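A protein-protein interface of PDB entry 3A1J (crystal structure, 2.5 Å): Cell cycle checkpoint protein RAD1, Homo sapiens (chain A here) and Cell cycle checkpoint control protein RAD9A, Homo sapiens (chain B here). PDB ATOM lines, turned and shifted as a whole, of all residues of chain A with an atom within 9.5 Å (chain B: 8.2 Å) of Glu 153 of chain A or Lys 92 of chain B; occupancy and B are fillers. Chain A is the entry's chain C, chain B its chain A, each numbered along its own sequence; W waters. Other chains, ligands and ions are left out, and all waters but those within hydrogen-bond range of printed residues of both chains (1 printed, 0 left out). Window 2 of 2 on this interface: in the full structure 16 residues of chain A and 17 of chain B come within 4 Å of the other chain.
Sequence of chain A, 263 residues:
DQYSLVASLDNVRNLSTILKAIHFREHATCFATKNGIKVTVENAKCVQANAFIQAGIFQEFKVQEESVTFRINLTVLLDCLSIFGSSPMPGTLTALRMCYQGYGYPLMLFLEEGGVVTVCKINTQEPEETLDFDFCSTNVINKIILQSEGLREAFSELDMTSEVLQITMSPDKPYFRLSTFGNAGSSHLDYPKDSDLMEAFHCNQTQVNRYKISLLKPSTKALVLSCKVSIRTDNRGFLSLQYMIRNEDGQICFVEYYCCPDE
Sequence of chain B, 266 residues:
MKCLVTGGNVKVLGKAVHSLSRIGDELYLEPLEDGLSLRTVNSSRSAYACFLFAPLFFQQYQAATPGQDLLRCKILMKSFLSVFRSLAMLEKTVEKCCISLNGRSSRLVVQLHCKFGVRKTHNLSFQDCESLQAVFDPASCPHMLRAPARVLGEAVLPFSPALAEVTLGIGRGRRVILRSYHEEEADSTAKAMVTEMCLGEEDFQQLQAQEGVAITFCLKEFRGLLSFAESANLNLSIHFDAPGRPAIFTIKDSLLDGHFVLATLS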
ATOM      1  N   GLN A 147       3.371  18.554 -15.050  1.00  0.00           N
ATOM      2  CA  GLN A 147       2.508  17.733 -15.875  1.00  0.00           C
ATOM      3  C   GLN A 147       1.187  18.515 -15.894  1.00  0.00           C
ATOM      4  O   GLN A 147       0.429  18.493 -14.924  1.00  0.00           O
ATOM      5  CB  GLN A 147       2.313  16.389 -15.192  1.00  0.00           C
ATOM      6  CG  GLN A 147       1.995  15.243 -16.104  1.00  0.00           C
ATOM      7  CD  GLN A 147       1.804  13.956 -15.325  1.00  0.00           C
ATOM      8  OE1 GLN A 147       0.785  13.769 -14.648  1.00  0.00           O
ATOM      9  NE2 GLN A 147       2.794  13.068 -15.401  1.00  0.00           N
ATOM     10  N   SER A 148       0.923  19.216 -16.990  1.00  0.00           N
ATOM     11  CA  SER A 148      -0.281  20.031 -17.118  1.00  0.00           C
ATOM     12  C   SER A 148      -1.587  19.384 -16.660  1.00  0.00           C
ATOM     13  O   SER A 148      -2.338  19.971 -15.884  1.00  0.00           O
ATOM     14  CB  SER A 148      -0.425  20.502 -18.565  1.00  0.00           C
ATOM     15  OG  SER A 148       0.687  21.295 -18.940  1.00  0.00           O
ATOM     16  N   GLU A 149      -1.857  18.179 -17.146  1.00  0.00           N
ATOM     17  CA  GLU A 149      -3.085  17.463 -16.804  1.00  0.00           C
ATOM     18  C   GLU A 149      -3.588  17.658 -15.368  1.00  0.00           C
ATOM     19  O   GLU A 149      -4.736  18.049 -15.161  1.00  0.00           O
ATOM     20  CB  GLU A 149      -2.914  15.960 -17.077  1.00  0.00           C
ATOM     21  CG  GLU A 149      -2.920  15.532 -18.560  1.00  0.00           C
ATOM     22  CD  GLU A 149      -1.719  16.035 -19.373  1.00  0.00           C
ATOM     23  OE1 GLU A 149      -0.566  15.954 -18.885  1.00  0.00           O
ATOM     24  OE2 GLU A 149      -1.935  16.494 -20.518  1.00  0.00           O
ATOM     25  N   GLY A 150      -2.737  17.396 -14.381  1.00  0.00           N
ATOM     26  CA  GLY A 150      -3.168  17.521 -12.999  1.00  0.00           C
ATOM     27  C   GLY A 150      -3.083  18.882 -12.330  1.00  0.00           C
ATOM     28  O   GLY A 150      -3.060  18.957 -11.102  1.00  0.00           O
ATOM     29  N   LEU A 151      -3.048  19.956 -13.114  1.00  0.00           N
ATOM     30  CA  LEU A 151      -2.964  21.303 -12.550  1.00  0.00           C
ATOM     31  C   LEU A 151      -4.185  22.136 -12.911  1.00  0.00           C
ATOM     32  O   LEU A 151      -4.469  23.152 -12.280  1.00  0.00           O
ATOM     33  CB  LEU A 151      -1.716  22.018 -13.066  1.00  0.00           C
ATOM     34  CG  LEU A 151      -0.386  21.270 -13.002  1.00  0.00           C
ATOM     35  CD1 LEU A 151       0.709  22.204 -13.472  1.00  0.00           C
ATOM     36  CD2 LEU A 151      -0.105  20.781 -11.587  1.00  0.00           C
ATOM     37  N   ARG A 152      -4.903  21.693 -13.933  1.00  0.00           N
ATOM     38  CA  ARG A 152      -6.087  22.391 -14.417  1.00  0.00           C
ATOM     39  C   ARG A 152      -7.147  22.678 -13.352  1.00  0.00           C
ATOM     40  O   ARG A 152      -7.531  23.830 -13.154  1.00  0.00           O
ATOM     41  CB  ARG A 152      -6.689  21.591 -15.574  1.00  0.00           C
ATOM     42  CG  ARG A 152      -5.683  21.353 -16.690  1.00  0.00           C
ATOM     43  CD  ARG A 152      -6.199  20.400 -17.751  1.00  0.00           C
ATOM     44  NE  ARG A 152      -5.193  20.174 -18.786  1.00  0.00           N
ATOM     45  CZ  ARG A 152      -5.295  19.253 -19.739  1.00  0.00           C
ATOM     46  NH1 ARG A 152      -6.362  18.465 -19.791  1.00  0.00           N
ATOM     47  NH2 ARG A 152      -4.329  19.116 -20.638  1.00  0.00           N
ATOM     48  N   GLU A 153      -7.622  21.644 -12.668  1.00  0.00           N
ATOM     49  CA  GLU A 153      -8.632  21.845 -11.637  1.00  0.00           C
ATOM     50  C   GLU A 153      -8.117  22.839 -10.610  1.00  0.00           C
ATOM     51  O   GLU A 153      -8.750  23.856 -10.342  1.00  0.00           O
ATOM     52  CB  GLU A 153      -8.962  20.534 -10.924  1.00  0.00           C
ATOM     53  CG  GLU A 153      -9.373  19.395 -11.833  1.00  0.00           C
ATOM     54  CD  GLU A 153     -10.135  18.316 -11.082  1.00  0.00           C
ATOM     55  OE1 GLU A 153     -11.323  18.544 -10.771  1.00  0.00           O
ATOM     56  OE2 GLU A 153      -9.551  17.246 -10.794  1.00  0.00           O
ATOM     57  N   ALA A 154      -6.958  22.538 -10.040  1.00  0.00           N
ATOM     58  CA  ALA A 154      -6.354  23.397  -9.034  1.00  0.00           C
ATOM     59  C   ALA A 154      -6.151  24.844  -9.498  1.00  0.00           C
ATOM     60  O   ALA A 154      -6.500  25.780  -8.778  1.00  0.00           O
ATOM     61  CB  ALA A 154      -5.024  22.798  -8.574  1.00  0.00           C
ATOM     62  N   PHE A 155      -5.597  25.034 -10.693  1.00  0.00           N
ATOM     63  CA  PHE A 155      -5.355  26.382 -11.191  1.00  0.00           C
ATOM     64  C   PHE A 155      -6.618  27.205 -11.424  1.00  0.00           C
ATOM     65  O   PHE A 155      -6.579  28.437 -11.338  1.00  0.00           O
ATOM     66  CB  PHE A 155      -4.526  26.351 -12.482  1.00  0.00           C
ATOM     67  CG  PHE A 155      -3.035  26.237 -12.254  1.00  0.00           C
ATOM     68  CD1 PHE A 155      -2.141  26.923 -13.079  1.00  0.00           C
ATOM     69  CD2 PHE A 155      -2.520  25.427 -11.241  1.00  0.00           C
ATOM     70  CE1 PHE A 155      -0.765  26.804 -12.901  1.00  0.00           C
ATOM     71  CE2 PHE A 155      -1.142  25.302 -11.057  1.00  0.00           C
ATOM     72  CZ  PHE A 155      -0.265  25.989 -11.887  1.00  0.00           C
ATOM     73  N   SER A 156      -7.737  26.544 -11.717  1.00  0.00           N
ATOM     74  CA  SER A 156      -8.981  27.274 -11.942  1.00  0.00           C
ATOM     75  C   SER A 156      -9.632  27.677 -10.615  1.00  0.00           C
ATOM     76  O   SER A 156     -10.597  28.446 -10.599  1.00  0.00           O
ATOM     77  CB  SER A 156      -9.967  26.435 -12.757  1.00  0.00           C
ATOM     78  OG  SER A 156     -10.685  25.545 -11.923  1.00  0.00           O
ATOM     79  N   GLU A 157      -9.105  27.162  -9.505  1.00  0.00           N
ATOM     80  CA  GLU A 157      -9.644  27.493  -8.189  1.00  0.00           C
ATOM     81  C   GLU A 157      -8.818  28.534  -7.437  1.00  0.00           C
ATOM     82  O   GLU A 157      -8.887  28.634  -6.209  1.00  0.00           O
ATOM     83  CB  GLU A 157      -9.805  26.226  -7.338  1.00  0.00           C
ATOM     84  CG  GLU A 157     -11.051  25.423  -7.696  1.00  0.00           C
ATOM     85  CD  GLU A 157     -12.309  26.289  -7.714  1.00  0.00           C
ATOM     86  OE1 GLU A 157     -12.625  26.900  -6.669  1.00  0.00           O
ATOM     87  OE2 GLU A 157     -12.978  26.366  -8.771  1.00  0.00           O
ATOM     88  N   LEU A 158      -8.041  29.307  -8.191  1.00  0.00           N
ATOM     89  CA  LEU A 158      -7.208  30.370  -7.635  1.00  0.00           C
ATOM     90  C   LEU A 158      -8.108  31.551  -7.321  1.00  0.00           C
ATOM     91  O   LEU A 158      -8.783  32.080  -8.205  1.00  0.00           O
ATOM     92  CB  LEU A 158      -6.141  30.791  -8.650  1.00  0.00           C
ATOM     93  CG  LEU A 158      -4.711  30.258  -8.507  1.00  0.00           C
ATOM     94  CD1 LEU A 158      -4.689  28.914  -7.794  1.00  0.00           C
ATOM     95  CD2 LEU A 158      -4.086  30.162  -9.897  1.00  0.00           C
ATOM     96  N   ASP A 159      -8.115  31.959  -6.057  1.00  0.00           N
ATOM     97  CA  ASP A 159      -8.944  33.071  -5.608  1.00  0.00           C
ATOM     98  C   ASP A 159      -8.754  34.344  -6.435  1.00  0.00           C
ATOM     99  O   ASP A 159      -7.837  35.126  -6.184  1.00  0.00           O
ATOM    100  CB  ASP A 159      -8.660  33.375  -4.139  1.00  0.00           C
ATOM    101  CG  ASP A 159      -9.595  34.419  -3.576  1.00  0.00           C
ATOM    102  OD1 ASP A 159     -10.350  35.012  -4.373  1.00  0.00           O
ATOM    103  OD2 ASP A 159      -9.575  34.647  -2.345  1.00  0.00           O
ATOM    104  N   LEU A 189      -0.941  27.185  -2.421  1.00  0.00           N
ATOM    105  CA  LEU A 189      -0.978  25.960  -3.218  1.00  0.00           C
ATOM    106  C   LEU A 189       0.465  25.469  -3.273  1.00  0.00           C
ATOM    107  O   LEU A 189       1.338  26.142  -3.819  1.00  0.00           O
ATOM    108  CB  LEU A 189      -1.517  26.253  -4.620  1.00  0.00           C
ATOM    109  CG  LEU A 189      -1.798  25.101  -5.591  1.00  0.00           C
ATOM    110  CD1 LEU A 189      -2.564  23.973  -4.906  1.00  0.00           C
ATOM    111  CD2 LEU A 189      -2.602  25.645  -6.766  1.00  0.00           C
ATOM    112  N   TYR A 191       3.410  22.496  -4.195  1.00  0.00           N
ATOM    113  CA  TYR A 191       3.818  21.350  -5.007  1.00  0.00           C
ATOM    114  C   TYR A 191       5.205  20.904  -4.536  1.00  0.00           C
ATOM    115  O   TYR A 191       6.176  21.645  -4.671  1.00  0.00           O
ATOM    116  CB  TYR A 191       3.869  21.743  -6.486  1.00  0.00           C
ATOM    117  CG  TYR A 191       2.511  22.003  -7.091  1.00  0.00           C
ATOM    118  CD1 TYR A 191       1.782  20.973  -7.687  1.00  0.00           C
ATOM    119  CD2 TYR A 191       1.931  23.271  -7.031  1.00  0.00           C
ATOM    120  CE1 TYR A 191       0.509  21.200  -8.208  1.00  0.00           C
ATOM    121  CE2 TYR A 191       0.656  23.508  -7.549  1.00  0.00           C
ATOM    122  CZ  TYR A 191      -0.048  22.468  -8.135  1.00  0.00           C
ATOM    123  OH  TYR A 191      -1.311  22.697  -8.632  1.00  0.00           O
ATOM    124  N   THR A 220      -4.654  30.356 -18.692  1.00  0.00           N
ATOM    125  CA  THR A 220      -5.384  29.116 -18.438  1.00  0.00           C
ATOM    126  C   THR A 220      -5.780  28.391 -19.732  1.00  0.00           C
ATOM    127  O   THR A 220      -5.763  27.155 -19.795  1.00  0.00           O
ATOM    128  CB  THR A 220      -6.666  29.399 -17.620  1.00  0.00           C
ATOM    129  OG1 THR A 220      -6.301  29.796 -16.295  1.00  0.00           O
ATOM    130  CG2 THR A 220      -7.548  28.155 -17.544  1.00  0.00           C
ATOM    131  N   LEU A 223      -3.015  26.334 -20.830  1.00  0.00           N
ATOM    132  CA  LEU A 223      -2.796  25.241 -19.885  1.00  0.00           C
ATOM    133  C   LEU A 223      -3.687  24.036 -20.183  1.00  0.00           C
ATOM    134  O   LEU A 223      -3.232  22.891 -20.185  1.00  0.00           O
ATOM    135  CB  LEU A 223      -3.066  25.718 -18.455  1.00  0.00           C
ATOM    136  CG  LEU A 223      -3.087  24.687 -17.317  1.00  0.00           C
ATOM    137  CD1 LEU A 223      -1.720  24.044 -17.122  1.00  0.00           C
ATOM    138  CD2 LEU A 223      -3.511  25.394 -16.048  1.00  0.00           C
ATOM    139  N   VAL A 224      -4.962  24.310 -20.431  1.00  0.00           N
ATOM    140  CA  VAL A 224      -5.938  23.269 -20.715  1.00  0.00           C
ATOM    141  C   VAL A 224      -5.569  22.377 -21.898  1.00  0.00           C
ATOM    142  O   VAL A 224      -5.783  21.166 -21.859  1.00  0.00           O
ATOM    143  CB  VAL A 224      -7.322  23.884 -20.984  1.00  0.00           C
ATOM    144  CG1 VAL A 224      -8.341  22.783 -21.214  1.00  0.00           C
ATOM    145  CG2 VAL A 224      -7.738  24.750 -19.805  1.00  0.00           C
ATOM    146  N   VAL B  10     -15.525  13.641   2.575  1.00  0.00           N
ATOM    147  CA  VAL B  10     -15.068  14.973   2.244  1.00  0.00           C
ATOM    148  C   VAL B  10     -16.067  15.556   1.264  1.00  0.00           C
ATOM    149  O   VAL B  10     -16.499  16.702   1.413  1.00  0.00           O
ATOM    150  CB  VAL B  10     -13.667  14.979   1.613  1.00  0.00           C
ATOM    151  CG1 VAL B  10     -13.616  14.024   0.455  1.00  0.00           C
ATOM    152  CG2 VAL B  10     -13.328  16.386   1.138  1.00  0.00           C
ATOM    153  N   LYS B  11     -16.461  14.764   0.275  1.00  0.00           N
ATOM    154  CA  LYS B  11     -17.419  15.254  -0.694  1.00  0.00           C
ATOM    155  C   LYS B  11     -18.765  15.558  -0.038  1.00  0.00           C
ATOM    156  O   LYS B  11     -19.428  16.530  -0.416  1.00  0.00           O
ATOM    157  CB  LYS B  11     -17.627  14.254  -1.827  1.00  0.00           C
ATOM    158  CG  LYS B  11     -18.540  14.794  -2.919  1.00  0.00           C
ATOM    159  CD  LYS B  11     -18.985  13.702  -3.894  1.00  0.00           C
ATOM    160  CE  LYS B  11     -19.887  14.277  -4.981  1.00  0.00           C
ATOM    161  NZ  LYS B  11     -20.611  13.219  -5.748  1.00  0.00           N
ATOM    162  N   ARG B  85     -15.965  24.935  -3.230  1.00  0.00           N
ATOM    163  CA  ARG B  85     -16.631  25.379  -4.453  1.00  0.00           C
ATOM    164  C   ARG B  85     -16.790  24.298  -5.529  1.00  0.00           C
ATOM    165  O   ARG B  85     -17.904  24.001  -5.956  1.00  0.00           O
ATOM    166  CB  ARG B  85     -15.865  26.567  -5.036  1.00  0.00           C
ATOM    167  CG  ARG B  85     -16.456  27.165  -6.307  1.00  0.00           C
ATOM    168  CD  ARG B  85     -15.448  28.127  -6.936  1.00  0.00           C
ATOM    169  NE  ARG B  85     -15.901  28.711  -8.200  1.00  0.00           N
ATOM    170  CZ  ARG B  85     -15.102  29.350  -9.054  1.00  0.00           C
ATOM    171  NH1 ARG B  85     -13.807  29.482  -8.780  1.00  0.00           N
ATOM    172  NH2 ARG B  85     -15.592  29.859 -10.180  1.00  0.00           N
ATOM    173  N   SER B  86     -15.681  23.712  -5.967  1.00  0.00           N
ATOM    174  CA  SER B  86     -15.725  22.688  -7.011  1.00  0.00           C
ATOM    175  C   SER B  86     -15.870  21.256  -6.511  1.00  0.00           C
ATOM    176  O   SER B  86     -14.879  20.574  -6.271  1.00  0.00           O
ATOM    177  CB  SER B  86     -14.474  22.771  -7.885  1.00  0.00           C
ATOM    178  OG  SER B  86     -14.428  21.672  -8.779  1.00  0.00           O
ATOM    179  N   LEU B  87     -17.109  20.798  -6.376  1.00  0.00           N
ATOM    180  CA  LEU B  87     -17.367  19.439  -5.918  1.00  0.00           C
ATOM    181  C   LEU B  87     -16.686  18.424  -6.839  1.00  0.00           C
ATOM    182  O   LEU B  87     -16.533  17.250  -6.493  1.00  0.00           O
ATOM    183  CB  LEU B  87     -18.877  19.196  -5.861  1.00  0.00           C
ATOM    184  CG  LEU B  87     -19.614  20.085  -4.849  1.00  0.00           C
ATOM    185  CD1 LEU B  87     -21.109  20.026  -5.111  1.00  0.00           C
ATOM    186  CD2 LEU B  87     -19.284  19.646  -3.426  1.00  0.00           C
ATOM    187  N   ALA B  88     -16.278  18.882  -8.017  1.00  0.00           N
ATOM    188  CA  ALA B  88     -15.594  18.018  -8.962  1.00  0.00           C
ATOM    189  C   ALA B  88     -14.172  17.832  -8.457  1.00  0.00           C
ATOM    190  O   ALA B  88     -13.747  16.721  -8.155  1.00  0.00           O
ATOM    191  CB  ALA B  88     -15.580  18.659 -10.334  1.00  0.00           C
ATOM    192  N   MET B  89     -13.450  18.944  -8.362  1.00  0.00           N
ATOM    193  CA  MET B  89     -12.069  18.955  -7.898  1.00  0.00           C
ATOM    194  C   MET B  89     -11.945  18.224  -6.567  1.00  0.00           C
ATOM    195  O   MET B  89     -10.879  17.714  -6.225  1.00  0.00           O
ATOM    196  CB  MET B  89     -11.584  20.405  -7.781  1.00  0.00           C
ATOM    197  CG  MET B  89     -10.146  20.584  -7.315  1.00  0.00           C
ATOM    198  SD  MET B  89     -10.037  21.036  -5.431  1.00  0.00           S
ATOM    199  CE  MET B  89     -10.080  22.969  -5.574  1.00  0.00           C
ATOM    200  N   LEU B  90     -13.042  18.173  -5.817  1.00  0.00           N
ATOM    201  CA  LEU B  90     -13.042  17.470  -4.543  1.00  0.00           C
ATOM    202  C   LEU B  90     -13.017  15.994  -4.870  1.00  0.00           C
ATOM    203  O   LEU B  90     -11.994  15.330  -4.730  1.00  0.00           O
ATOM    204  CB  LEU B  90     -14.310  17.768  -3.731  1.00  0.00           C
ATOM    205  CG  LEU B  90     -14.435  19.057  -2.917  1.00  0.00           C
ATOM    206  CD1 LEU B  90     -15.596  18.902  -1.949  1.00  0.00           C
ATOM    207  CD2 LEU B  90     -13.155  19.327  -2.144  1.00  0.00           C
ATOM    208  N   GLU B  91     -14.168  15.503  -5.320  1.00  0.00           N
ATOM    209  CA  GLU B  91     -14.369  14.110  -5.688  1.00  0.00           C
ATOM    210  C   GLU B  91     -13.123  13.426  -6.245  1.00  0.00           C
ATOM    211  O   GLU B  91     -12.846  12.269  -5.919  1.00  0.00           O
ATOM    212  CB  GLU B  91     -15.516  14.029  -6.702  1.00  0.00           C
ATOM    213  CG  GLU B  91     -15.867  12.624  -7.171  1.00  0.00           C
ATOM    214  CD  GLU B  91     -17.303  12.521  -7.666  1.00  0.00           C
ATOM    215  OE1 GLU B  91     -17.674  11.464  -8.218  1.00  0.00           O
ATOM    216  OE2 GLU B  91     -18.069  13.496  -7.493  1.00  0.00           O
ATOM    217  N   LYS B  92     -12.368  14.148  -7.071  1.00  0.00           N
ATOM    218  CA  LYS B  92     -11.159  13.608  -7.687  1.00  0.00           C
ATOM    219  C   LYS B  92      -9.857  13.765  -6.898  1.00  0.00           C
ATOM    220  O   LYS B  92      -9.411  12.834  -6.222  1.00  0.00           O
ATOM    221  CB  LYS B  92     -10.954  14.226  -9.075  1.00  0.00           C
ATOM    222  CG  LYS B  92     -11.779  13.610 -10.198  1.00  0.00           C
ATOM    223  CD  LYS B  92     -11.325  14.185 -11.538  1.00  0.00           C
ATOM    224  CE  LYS B  92     -11.961  13.476 -12.727  1.00  0.00           C
ATOM    225  NZ  LYS B  92     -11.437  14.002 -14.023  1.00  0.00           N
ATOM    226  N   THR B  93      -9.265  14.954  -6.995  1.00  0.00           N
ATOM    227  CA  THR B  93      -7.981  15.278  -6.372  1.00  0.00           C
ATOM    228  C   THR B  93      -7.834  15.330  -4.848  1.00  0.00           C
ATOM    229  O   THR B  93      -6.748  15.073  -4.335  1.00  0.00           O
ATOM    230  CB  THR B  93      -7.457  16.616  -6.914  1.00  0.00           C
ATOM    231  OG1 THR B  93      -8.244  17.685  -6.378  1.00  0.00           O
ATOM    232  CG2 THR B  93      -7.565  16.655  -8.427  1.00  0.00           C
ATOM    233  N   VAL B  94      -8.901  15.661  -4.126  1.00  0.00           N
ATOM    234  CA  VAL B  94      -8.827  15.771  -2.670  1.00  0.00           C
ATOM    235  C   VAL B  94      -8.971  14.454  -1.909  1.00  0.00           C
ATOM    236  O   VAL B  94      -9.953  13.733  -2.066  1.00  0.00           O
ATOM    237  CB  VAL B  94      -9.894  16.749  -2.120  1.00  0.00           C
ATOM    238  CG1 VAL B  94      -9.697  16.943  -0.622  1.00  0.00           C
ATOM    239  CG2 VAL B  94      -9.817  18.082  -2.848  1.00  0.00           C
ATOM    240  N   GLU B  95      -7.997  14.155  -1.059  1.00  0.00           N
ATOM    241  CA  GLU B  95      -8.033  12.932  -0.274  1.00  0.00           C
ATOM    242  C   GLU B  95      -8.408  13.191   1.184  1.00  0.00           C
ATOM    243  O   GLU B  95      -9.258  12.500   1.745  1.00  0.00           O
ATOM    244  CB  GLU B  95      -6.680  12.229  -0.357  1.00  0.00           C
ATOM    245  CG  GLU B  95      -6.311  11.851  -1.778  1.00  0.00           C
ATOM    246  CD  GLU B  95      -4.975  11.162  -1.863  1.00  0.00           C
ATOM    247  OE1 GLU B  95      -3.988  11.720  -1.331  1.00  0.00           O
ATOM    248  OE2 GLU B  95      -4.908  10.069  -2.467  1.00  0.00           O
ATOM    249  N   HIS B 113      -5.546  17.904   1.559  1.00  0.00           N
ATOM    250  CA  HIS B 113      -4.399  17.083   1.198  1.00  0.00           C
ATOM    251  C   HIS B 113      -4.790  16.393  -0.099  1.00  0.00           C
ATOM    252  O   HIS B 113      -5.632  15.493  -0.106  1.00  0.00           O
ATOM    253  CB  HIS B 113      -4.104  16.064   2.297  1.00  0.00           C
ATOM    254  CG  HIS B 113      -3.611  16.684   3.567  1.00  0.00           C
ATOM    255  ND1 HIS B 113      -2.379  17.296   3.667  1.00  0.00           N
ATOM    256  CD2 HIS B 113      -4.202  16.830   4.778  1.00  0.00           C
ATOM    257  CE1 HIS B 113      -2.235  17.794   4.882  1.00  0.00           C
ATOM    258  NE2 HIS B 113      -3.326  17.526   5.576  1.00  0.00           N
ATOM    259  N   CYS B 114      -4.174  16.831  -1.195  1.00  0.00           N
ATOM    260  CA  CYS B 114      -4.478  16.303  -2.526  1.00  0.00           C
ATOM    261  C   CYS B 114      -3.524  15.249  -3.076  1.00  0.00           C
ATOM    262  O   CYS B 114      -2.452  15.014  -2.530  1.00  0.00           O
ATOM    263  CB  CYS B 114      -4.556  17.465  -3.513  1.00  0.00           C
ATOM    264  SG  CYS B 114      -5.613  18.791  -2.940  1.00  0.00           S
ATOM    265  N   LYS B 115      -3.932  14.625  -4.174  1.00  0.00           N
ATOM    266  CA  LYS B 115      -3.121  13.606  -4.824  1.00  0.00           C
ATOM    267  C   LYS B 115      -1.744  14.131  -5.179  1.00  0.00           C
ATOM    268  O   LYS B 115      -1.526  15.337  -5.257  1.00  0.00           O
ATOM    269  CB  LYS B 115      -3.792  13.129  -6.112  1.00  0.00           C
ATOM    270  CG  LYS B 115      -4.928  12.152  -5.924  1.00  0.00           C
ATOM    271  CD  LYS B 115      -5.551  11.814  -7.264  1.00  0.00           C
ATOM    272  CE  LYS B 115      -6.712  10.848  -7.099  1.00  0.00           C
ATOM    273  NZ  LYS B 115      -7.502  10.707  -8.359  1.00  0.00           N
ATOM    274  N   PHE B 116      -0.816  13.207  -5.393  1.00  0.00           N
ATOM    275  CA  PHE B 116       0.544  13.547  -5.789  1.00  0.00           C
ATOM    276  C   PHE B 116       1.240  14.494  -4.838  1.00  0.00           C
ATOM    277  O   PHE B 116       2.086  15.284  -5.249  1.00  0.00           O
ATOM    278  CB  PHE B 116       0.528  14.146  -7.197  1.00  0.00           C
ATOM    279  CG  PHE B 116      -0.234  13.312  -8.195  1.00  0.00           C
ATOM    280  CD1 PHE B 116       0.162  12.003  -8.476  1.00  0.00           C
ATOM    281  CD2 PHE B 116      -1.350  13.830  -8.846  1.00  0.00           C
ATOM    282  CE1 PHE B 116      -0.545  11.218  -9.392  1.00  0.00           C
ATOM    283  CE2 PHE B 116      -2.066  13.057  -9.765  1.00  0.00           C
ATOM    284  CZ  PHE B 116      -1.661  11.746 -10.039  1.00  0.00           C
ATOM    285  N   LYS B 120      -3.205  22.188  -0.403  1.00  0.00           N
ATOM    286  CA  LYS B 120      -3.774  23.521  -0.512  1.00  0.00           C
ATOM    287  C   LYS B 120      -4.224  23.969   0.860  1.00  0.00           C
ATOM    288  O   LYS B 120      -5.049  23.310   1.486  1.00  0.00           O
ATOM    289  CB  LYS B 120      -4.974  23.549  -1.462  1.00  0.00           C
ATOM    290  CG  LYS B 120      -5.410  24.970  -1.809  1.00  0.00           C
ATOM    291  CD  LYS B 120      -6.713  25.016  -2.595  1.00  0.00           C
ATOM    292  CE  LYS B 120      -7.047  26.453  -3.018  1.00  0.00           C
ATOM    293  NZ  LYS B 120      -8.460  26.589  -3.524  1.00  0.00           N
HETATM  294  O   HOH W   1      -6.542  25.830  -6.187  1.00  0.00           O
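Of the 18 printed residues of chain A, 3 touch a printed residue of chain B. Along chain B the printed residues that touch a printed residue of chain A span positions 85 to 120. Among the printed residues, Asp or Glu carboxylates within 4 Å of a Lys or Arg side-chain nitrogen of the other chain: Glu 157 of chain A with Arg 85 of chain B (3.2 Å).
The backbone NH (N) of Lys 115 of chain B is in hydrogen-bond range of the backbone carbonyl oxygen (O) of Thr 93 of chain B (2.9 Å). The backbone carbonyl oxygen of Met 89 of chain B is in hydrogen-bond range of the side-chain hydroxyl of Thr 93 of chain B, 2.6 Å away. O of Glu 153 of chain A lies within hydrogen-bond range of OG of Ser 156 of chain A, 3.0 Å away. N of Ala 88 of chain B lies close to OG of Ser 86 of chain B, 3.4 Å away. OG of Ser 86 of chain B lies within hydrogen-bond range of N of Met 89 of chain B.
Water W1 lies within hydrogen-bond range of O of Ala 154 of chain A (2.6 Å) and NZ of Lys 120 of chain B (3.4 Å).
Of chain B, only Ala 88, Met 89, Lys 92 and Thr 93 come within 4 Å of Glu 153 of chain A. Of the printed residues of chain A, Lys 92 of chain B touches Glu 153. No residue of chain B comes within 4 Å of Ala 154 of chain A. Of chain A, only Glu 153 comes within 4 Å of Thr 93 of chain B. Printed residues of chain A within 4 Å of Met 89 of chain B: Glu 153 (3.0 Å) and Glu 157 (3.4 Å). Printed residues of chain A within 4 Å of Lys 120 of chain B: Glu 157 (3.4 Å). Of the printed residues of chain A, Arg 85 of chain B touches Ser 156 and Glu 157. Printed residues of chain A within 4 Å of Ser 86 of chain B: Glu 157 (3.99 Å). Of the printed residues of chain B, Glu 157 of chain A touches Arg 85 (3.1 Å), Ser 86 (3.99 Å), Met 89 (3.4 Å) and Lys 120 (3.4 Å). Gln 147 of chain A touches none of the printed residues of chain B. The nearest residue of chain A that does not touch Lys 92 of chain B is Glu 149 of chain A (7.9 Å). The nearest printed residue of chain A that does not touch Ser 86 of chain B is Glu 153 of chain A (4.8 Å).
Glu 153 of chain A touches Ala 88 of chain B (OE1 to C, 3.7 Å). Glu 153 of chain A touches Lys 92 of chain B. Thr 93 of chain B touches Glu 153 of chain A (CG2 to OE2, 3.1 Å). Ser 156 of chain A touches Arg 85 of chain B (O to NH1, 3.8 Å). Ser 86 of chain B touches Glu 157 of chain A. Met 89 of chain B touches Glu 157 of chain A.
The side-chain amino group (NZ) of Lys 120 of chain B sits at hydrogen-bond distance from the backbone carbonyl oxygen (O) of Glu 157 of chain A. N of Met 89 of chain B lies close to OE1 of Glu 153 of chain A, at 3.2 Å. The guanidinium group (NH1) of Arg 85 of chain B lies within salt-bridge range of the side-chain carboxylate (OE2) of Glu 157 of chain A.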
